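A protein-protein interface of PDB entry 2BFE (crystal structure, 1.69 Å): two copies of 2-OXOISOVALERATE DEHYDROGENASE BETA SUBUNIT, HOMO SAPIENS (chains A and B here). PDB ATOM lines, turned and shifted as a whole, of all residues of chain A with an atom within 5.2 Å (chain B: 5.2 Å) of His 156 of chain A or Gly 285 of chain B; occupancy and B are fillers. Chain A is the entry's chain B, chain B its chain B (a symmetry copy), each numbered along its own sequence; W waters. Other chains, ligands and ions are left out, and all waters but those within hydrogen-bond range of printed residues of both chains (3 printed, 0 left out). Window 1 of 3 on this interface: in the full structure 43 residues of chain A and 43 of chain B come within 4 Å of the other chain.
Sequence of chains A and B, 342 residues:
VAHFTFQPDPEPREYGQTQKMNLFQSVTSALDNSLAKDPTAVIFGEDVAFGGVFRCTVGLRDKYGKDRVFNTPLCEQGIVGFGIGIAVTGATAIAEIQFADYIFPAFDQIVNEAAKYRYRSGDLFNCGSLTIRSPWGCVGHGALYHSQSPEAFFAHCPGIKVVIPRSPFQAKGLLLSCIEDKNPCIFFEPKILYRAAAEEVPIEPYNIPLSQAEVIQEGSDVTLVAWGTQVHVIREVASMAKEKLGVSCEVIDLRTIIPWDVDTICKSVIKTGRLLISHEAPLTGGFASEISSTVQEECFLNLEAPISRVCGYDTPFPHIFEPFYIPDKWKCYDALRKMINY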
ATOM      1  N   ALA A 152     -23.444 -20.944  -1.734  1.00  0.00           N
ATOM      2  CA  ALA A 152     -23.953 -19.590  -2.040  1.00  0.00           C
ATOM      3  C   ALA A 152     -24.933 -19.595  -3.198  1.00  0.00           C
ATOM      4  O   ALA A 152     -25.798 -18.709  -3.277  1.00  0.00           O
ATOM      5  CB  ALA A 152     -22.794 -18.608  -2.315  1.00  0.00           C
ATOM      6  N   PHE A 153     -24.815 -20.560  -4.111  1.00  0.00           N
ATOM      7  CA  PHE A 153     -25.786 -20.641  -5.233  1.00  0.00           C
ATOM      8  C   PHE A 153     -27.146 -20.969  -4.616  1.00  0.00           C
ATOM      9  O   PHE A 153     -28.137 -20.372  -5.009  1.00  0.00           O
ATOM     10  CB  PHE A 153     -25.410 -21.755  -6.207  1.00  0.00           C
ATOM     11  CG  PHE A 153     -24.164 -21.443  -7.024  1.00  0.00           C
ATOM     12  CD1 PHE A 153     -24.181 -20.357  -7.937  1.00  0.00           C
ATOM     13  CD2 PHE A 153     -23.002 -22.236  -6.911  1.00  0.00           C
ATOM     14  CE1 PHE A 153     -23.011 -20.041  -8.756  1.00  0.00           C
ATOM     15  CE2 PHE A 153     -21.860 -21.968  -7.720  1.00  0.00           C
ATOM     16  CZ  PHE A 153     -21.847 -20.839  -8.662  1.00  0.00           C
ATOM     17  N   PHE A 154     -27.187 -21.840  -3.611  1.00  0.00           N
ATOM     18  CA  PHE A 154     -28.481 -22.247  -3.074  1.00  0.00           C
ATOM     19  C   PHE A 154     -29.028 -21.255  -2.059  1.00  0.00           C
ATOM     20  O   PHE A 154     -30.233 -21.172  -1.817  1.00  0.00           O
ATOM     21  CB  PHE A 154     -28.332 -23.669  -2.482  1.00  0.00           C
ATOM     22  CG  PHE A 154     -28.136 -24.697  -3.548  1.00  0.00           C
ATOM     23  CD1 PHE A 154     -29.221 -25.067  -4.363  1.00  0.00           C
ATOM     24  CD2 PHE A 154     -26.840 -25.195  -3.804  1.00  0.00           C
ATOM     25  CE1 PHE A 154     -28.996 -25.986  -5.419  1.00  0.00           C
ATOM     26  CE2 PHE A 154     -26.641 -26.118  -4.832  1.00  0.00           C
ATOM     27  CZ  PHE A 154     -27.739 -26.475  -5.636  1.00  0.00           C
ATOM     28  N   ALA A 155     -28.122 -20.487  -1.456  1.00  0.00           N
ATOM     29  CA  ALA A 155     -28.538 -19.529  -0.398  1.00  0.00           C
ATOM     30  C   ALA A 155     -29.508 -18.470  -0.892  1.00  0.00           C
ATOM     31  O   ALA A 155     -30.193 -17.849  -0.095  1.00  0.00           O
ATOM     32  CB  ALA A 155     -27.290 -18.841   0.206  1.00  0.00           C
ATOM     33  N   HIS A 156     -29.495 -18.227  -2.197  1.00  0.00           N
ATOM     34  CA  HIS A 156     -30.376 -17.184  -2.791  1.00  0.00           C
ATOM     35  C   HIS A 156     -31.731 -17.741  -3.216  1.00  0.00           C
ATOM     36  O   HIS A 156     -32.498 -17.060  -3.896  1.00  0.00           O
ATOM     37  CB  HIS A 156     -29.630 -16.547  -3.972  1.00  0.00           C
ATOM     38  CG  HIS A 156     -30.381 -15.418  -4.621  1.00  0.00           C
ATOM     39  ND1 HIS A 156     -30.795 -14.315  -3.912  1.00  0.00           N
ATOM     40  CD2 HIS A 156     -30.720 -15.175  -5.915  1.00  0.00           C
ATOM     41  CE1 HIS A 156     -31.366 -13.446  -4.727  1.00  0.00           C
ATOM     42  NE2 HIS A 156     -31.404 -13.980  -5.938  1.00  0.00           N
ATOM     43  N   CYS A 157     -32.042 -18.961  -2.762  1.00  0.00           N
ATOM     44  CA  CYS A 157     -33.314 -19.666  -3.078  1.00  0.00           C
ATOM     45  C   CYS A 157     -34.215 -19.886  -1.830  1.00  0.00           C
ATOM     46  O   CYS A 157     -34.147 -20.920  -1.166  1.00  0.00           O
ATOM     47  CB  CYS A 157     -33.005 -20.995  -3.757  1.00  0.00           C
ATOM     48  SG  CYS A 157     -34.566 -21.697  -4.389  1.00  0.00           S
ATOM     49  N   PRO A 158     -35.134 -18.956  -1.567  1.00  0.00           N
ATOM     50  CA  PRO A 158     -36.133 -19.196  -0.506  1.00  0.00           C
ATOM     51  C   PRO A 158     -36.894 -20.549  -0.670  1.00  0.00           C
ATOM     52  O   PRO A 158     -37.371 -20.897  -1.774  1.00  0.00           O
ATOM     53  CB  PRO A 158     -37.078 -18.001  -0.685  1.00  0.00           C
ATOM     54  CG  PRO A 158     -36.137 -16.851  -1.228  1.00  0.00           C
ATOM     55  CD  PRO A 158     -35.316 -17.661  -2.229  1.00  0.00           C
ATOM     56  N   ILE A 258     -28.706 -21.491   5.151  1.00  0.00           N
ATOM     57  CA  ILE A 258     -30.053 -20.882   5.203  1.00  0.00           C
ATOM     58  C   ILE A 258     -31.098 -21.845   5.740  1.00  0.00           C
ATOM     59  O   ILE A 258     -31.050 -23.037   5.431  1.00  0.00           O
ATOM     60  CB  ILE A 258     -30.570 -20.325   3.832  1.00  0.00           C
ATOM     61  CG1 ILE A 258     -30.497 -21.372   2.683  1.00  0.00           C
ATOM     62  CG2 ILE A 258     -29.924 -18.963   3.470  1.00  0.00           C
ATOM     63  CD1 ILE A 258     -31.489 -20.955   1.537  1.00  0.00           C
ATOM     64  N   GLU A 290     -23.322 -12.129   2.499  1.00  0.00           N
ATOM     65  CA  GLU A 290     -24.624 -12.015   3.220  1.00  0.00           C
ATOM     66  C   GLU A 290     -24.447 -11.822   4.703  1.00  0.00           C
ATOM     67  O   GLU A 290     -25.119 -10.973   5.325  1.00  0.00           O
ATOM     68  CB  GLU A 290     -25.516 -13.244   2.953  1.00  0.00           C
ATOM     69  CG  GLU A 290     -26.945 -13.123   3.548  1.00  0.00           C
ATOM     70  CD  GLU A 290     -27.713 -11.900   3.075  1.00  0.00           C
ATOM     71  OE1 GLU A 290     -27.649 -11.626   1.882  1.00  0.00           O
ATOM     72  OE2 GLU A 290     -28.287 -11.188   3.920  1.00  0.00           O
ATOM     73  N   SER B 149     -35.446 -12.569 -11.317  1.00  0.00           N
ATOM     74  CA  SER B 149     -34.194 -11.869 -11.665  1.00  0.00           C
ATOM     75  C   SER B 149     -33.045 -12.682 -11.082  1.00  0.00           C
ATOM     76  O   SER B 149     -32.716 -12.510  -9.921  1.00  0.00           O
ATOM     77  CB  SER B 149     -34.170 -10.436 -11.076  1.00  0.00           C
ATOM     78  OG  SER B 149     -34.944 -10.369  -9.922  1.00  0.00           O
ATOM     79  N   ALA B 152     -27.999 -12.911  -9.114  1.00  0.00           N
ATOM     80  CA  ALA B 152     -27.133 -13.303  -7.983  1.00  0.00           C
ATOM     81  C   ALA B 152     -26.694 -14.753  -8.074  1.00  0.00           C
ATOM     82  O   ALA B 152     -25.632 -15.110  -7.540  1.00  0.00           O
ATOM     83  CB  ALA B 152     -27.824 -13.031  -6.630  1.00  0.00           C
ATOM     84  N   PHE B 153     -27.488 -15.606  -8.721  1.00  0.00           N
ATOM     85  CA  PHE B 153     -27.075 -17.024  -8.887  1.00  0.00           C
ATOM     86  C   PHE B 153     -25.836 -17.021  -9.782  1.00  0.00           C
ATOM     87  O   PHE B 153     -24.888 -17.734  -9.489  1.00  0.00           O
ATOM     88  CB  PHE B 153     -28.170 -17.840  -9.570  1.00  0.00           C
ATOM     89  CG  PHE B 153     -29.386 -18.073  -8.685  1.00  0.00           C
ATOM     90  CD1 PHE B 153     -29.252 -18.844  -7.501  1.00  0.00           C
ATOM     91  CD2 PHE B 153     -30.652 -17.561  -9.039  1.00  0.00           C
ATOM     92  CE1 PHE B 153     -30.403 -19.108  -6.638  1.00  0.00           C
ATOM     93  CE2 PHE B 153     -31.795 -17.830  -8.231  1.00  0.00           C
ATOM     94  CZ  PHE B 153     -31.679 -18.613  -6.992  1.00  0.00           C
ATOM     95  N   ALA B 281     -34.725  -8.757  -6.916  1.00  0.00           N
ATOM     96  CA  ALA B 281     -34.418 -10.079  -6.418  1.00  0.00           C
ATOM     97  C   ALA B 281     -34.529 -10.109  -4.894  1.00  0.00           C
ATOM     98  O   ALA B 281     -34.312  -9.054  -4.226  1.00  0.00           O
ATOM     99  CB  ALA B 281     -32.973 -10.489  -6.861  1.00  0.00           C
ATOM    100  N   PRO B 282     -34.815 -11.284  -4.330  1.00  0.00           N
ATOM    101  CA  PRO B 282     -34.815 -11.462  -2.901  1.00  0.00           C
ATOM    102  C   PRO B 282     -33.542 -10.995  -2.218  1.00  0.00           C
ATOM    103  O   PRO B 282     -32.433 -11.068  -2.798  1.00  0.00           O
ATOM    104  CB  PRO B 282     -34.909 -12.993  -2.747  1.00  0.00           C
ATOM    105  CG  PRO B 282     -35.789 -13.444  -3.909  1.00  0.00           C
ATOM    106  CD  PRO B 282     -35.197 -12.532  -5.037  1.00  0.00           C
ATOM    107  N   LEU B 283     -33.735 -10.480  -1.012  1.00  0.00           N
ATOM    108  CA  LEU B 283     -32.684  -9.941  -0.140  1.00  0.00           C
ATOM    109  C   LEU B 283     -31.541 -10.937   0.081  1.00  0.00           C
ATOM    110  O   LEU B 283     -30.377 -10.617  -0.201  1.00  0.00           O
ATOM    111  CB  LEU B 283     -33.317  -9.562   1.212  1.00  0.00           C
ATOM    112  CG  LEU B 283     -32.243  -9.011   2.201  1.00  0.00           C
ATOM    113  CD1 LEU B 283     -31.764  -7.603   1.834  1.00  0.00           C
ATOM    114  CD2 LEU B 283     -32.821  -9.045   3.608  1.00  0.00           C
ATOM    115  N   THR B 284     -31.872 -12.120   0.578  1.00  0.00           N
ATOM    116  CA  THR B 284     -30.821 -13.011   1.063  1.00  0.00           C
ATOM    117  C   THR B 284     -30.060 -13.596  -0.103  1.00  0.00           C
ATOM    118  O   THR B 284     -30.653 -14.239  -0.989  1.00  0.00           O
ATOM    119  CB  THR B 284     -31.419 -14.116   1.927  1.00  0.00           C
ATOM    120  OG1 THR B 284     -31.996 -13.517   3.084  1.00  0.00           O
ATOM    121  CG2 THR B 284     -30.340 -15.092   2.468  1.00  0.00           C
ATOM    122  N   GLY B 285     -28.742 -13.363  -0.091  1.00  0.00           N
ATOM    123  CA  GLY B 285     -27.880 -13.925  -1.201  1.00  0.00           C
ATOM    124  C   GLY B 285     -27.983 -13.085  -2.458  1.00  0.00           C
ATOM    125  O   GLY B 285     -27.333 -13.388  -3.467  1.00  0.00           O
ATOM    126  N   GLY B 286     -28.763 -12.002  -2.397  1.00  0.00           N
ATOM    127  CA  GLY B 286     -28.934 -11.064  -3.554  1.00  0.00           C
ATOM    128  C   GLY B 286     -27.659 -10.286  -3.800  1.00  0.00           C
ATOM    129  O   GLY B 286     -26.785 -10.259  -2.951  1.00  0.00           O
ATOM    130  N   PHE B 287     -27.522  -9.662  -4.963  1.00  0.00           N
ATOM    131  CA  PHE B 287     -26.246  -9.045  -5.284  1.00  0.00           C
ATOM    132  C   PHE B 287     -25.970  -7.800  -4.451  1.00  0.00           C
ATOM    133  O   PHE B 287     -24.816  -7.397  -4.298  1.00  0.00           O
ATOM    134  CB  PHE B 287     -26.114  -8.794  -6.811  1.00  0.00           C
ATOM    135  CG  PHE B 287     -24.680  -8.519  -7.223  1.00  0.00           C
ATOM    136  CD1 PHE B 287     -23.714  -9.530  -7.076  1.00  0.00           C
ATOM    137  CD2 PHE B 287     -24.287  -7.221  -7.610  1.00  0.00           C
ATOM    138  CE1 PHE B 287     -22.321  -9.298  -7.408  1.00  0.00           C
ATOM    139  CE2 PHE B 287     -22.896  -6.953  -7.913  1.00  0.00           C
ATOM    140  CZ  PHE B 287     -21.930  -7.988  -7.803  1.00  0.00           C
ATOM    141  N   SER B 289     -25.880  -7.765  -1.434  1.00  0.00           N
ATOM    142  CA  SER B 289     -25.054  -8.322  -0.350  1.00  0.00           C
ATOM    143  C   SER B 289     -23.548  -8.182  -0.642  1.00  0.00           C
ATOM    144  O   SER B 289     -22.767  -7.889   0.256  1.00  0.00           O
ATOM    145  CB  SER B 289     -25.455  -9.785  -0.104  1.00  0.00           C
ATOM    146  OG  SER B 289     -24.461 -10.483   0.608  1.00  0.00           O
ATOM    147  N   ARG B 309     -30.146  -2.087   2.176  1.00  0.00           N
ATOM    148  CA  ARG B 309     -30.521  -2.922   1.033  1.00  0.00           C
ATOM    149  C   ARG B 309     -32.040  -2.994   1.012  1.00  0.00           C
ATOM    150  O   ARG B 309     -32.643  -3.378   2.029  1.00  0.00           O
ATOM    151  CB  ARG B 309     -30.002  -4.338   1.203  1.00  0.00           C
ATOM    152  CG  ARG B 309     -28.506  -4.431   1.176  1.00  0.00           C
ATOM    153  CD  ARG B 309     -27.987  -5.883   1.335  1.00  0.00           C
ATOM    154  NE  ARG B 309     -28.234  -6.452   2.659  1.00  0.00           N
ATOM    155  CZ  ARG B 309     -28.296  -7.783   2.885  1.00  0.00           C
ATOM    156  NH1 ARG B 309     -28.228  -8.629   1.896  1.00  0.00           N
ATOM    157  NH2 ARG B 309     -28.474  -8.226   4.092  1.00  0.00           N
HETATM  158  O   HOH W   1     -30.618 -12.278  -8.167  1.00  0.00           O
HETATM  159  O   HOH W   2     -25.996 -16.012  -2.975  1.00  0.00           O
HETATM  160  O   HOH W   3     -33.860 -14.701  -7.461  1.00  0.00           O
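The side-chain hydroxyl of Ser 149 of chain B lies within hydrogen-bond range of the backbone NH of Ala 281 of chain B, 3.4 Å away.
His 156 of chain A touches just these residues of chain B: Ala 152 (3.7 Å), Phe 153 (3.6 Å), Ala 281 (3.9 Å), Pro 282 (3.2 Å), Thr 284 (2.9 Å), Gly 285 (3.4 Å) and Gly 286 (3.4 Å). Of the printed residues of chain A, Phe 153 of chain B touches Phe 153 and His 156. Of the printed residues of chain A, Ala 281 of chain B touches His 156 (3.9 Å). Of the printed residues of chain A, Leu 283 of chain B touches Glu 290 (3.6 Å). Gly 285 of chain B touches just these residues of chain A: His 156 (3.4 Å) and Glu 290 (2.8 Å). Printed residues of chain A within 4 Å of Gly 286 of chain B: His 156. Printed residues of chain A within 4 Å of Arg 309 of chain B: Glu 290. The nearest residue of chain A that does not touch Gly 285 of chain B is Ala 155 of chain A (4.7 Å).
Among the printed residues, 14 pairs touch across the chains. Among the printed residues, Asp or Glu carboxylates within 4 Å of a Lys or Arg side-chain nitrogen of the other chain: Glu 290 of chain A with Arg 309 of chain B.
Water W2 bridges O of Ala 152 of chain A (2.7 Å) and O of Gly 285 of chain B (3.0 Å). Water W1 lies within hydrogen-bond range of O of Ser 149 of chain B (2.7 Å), N of Ala 152 of chain B (2.9 Å) and NE2 of His 156 of chain A (2.9 Å). Water W3 lies within hydrogen-bond range of NE2 of His 156 of chain A and O of Ser 149 of chain B.
Phe 153 of chain B touches its own counterpart, Phe 153 of chain A. Positions printed for both chains: 152 and 153. Of the 14 pairs that touch across the chains among the printed residues, 1 has its exchanged pair printed and touching as well.
The side-chain carboxylate (OE1) of Glu 290 of chain A is in hydrogen-bond range of the backbone NH (N) of Gly 285 of chain B (2.8 Å). The backbone NH (N) of Glu 290 of chain A is in hydrogen-bond range of the side-chain hydroxyl (OG) of Ser 289 of chain B (2.8 Å). ND1 of His 156 of chain A lies within hydrogen-bond range of O of Thr 284 of chain B (2.9 Å). The backbone NH of Gly 286 of chain B lies within hydrogen-bond range of a ring nitrogen (ND1) of His 156 of chain A, 3.4 Å away. OE2 of Glu 290 of chain A lies within salt-bridge range of NH2 of Arg 309 of chain B, 3.0 Å away.
Among the printed residues, pairs that only touch across the chains: Phe 153 of chain A with Phe 153 of chain B (3.1 Å), His 156 of chain A with Pro 282 of chain B (3.2 Å), His 156 of chain A with Gly 285 of chain B (3.4 Å), Glu 290 of chain A with Thr 284 of chain B (3.6 Å), His 156 of chain A with Phe 153 of chain B (3.6 Å), Glu 290 of chain A with Leu 283 of chain B (3.6 Å), His 156 of chain A with Ala 152 of chain B (3.7 Å), Ala 155 of chain A with Thr 284 of chain B (3.7 Å) and His 156 of chain A with Ala 281 of chain B (3.9 Å).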
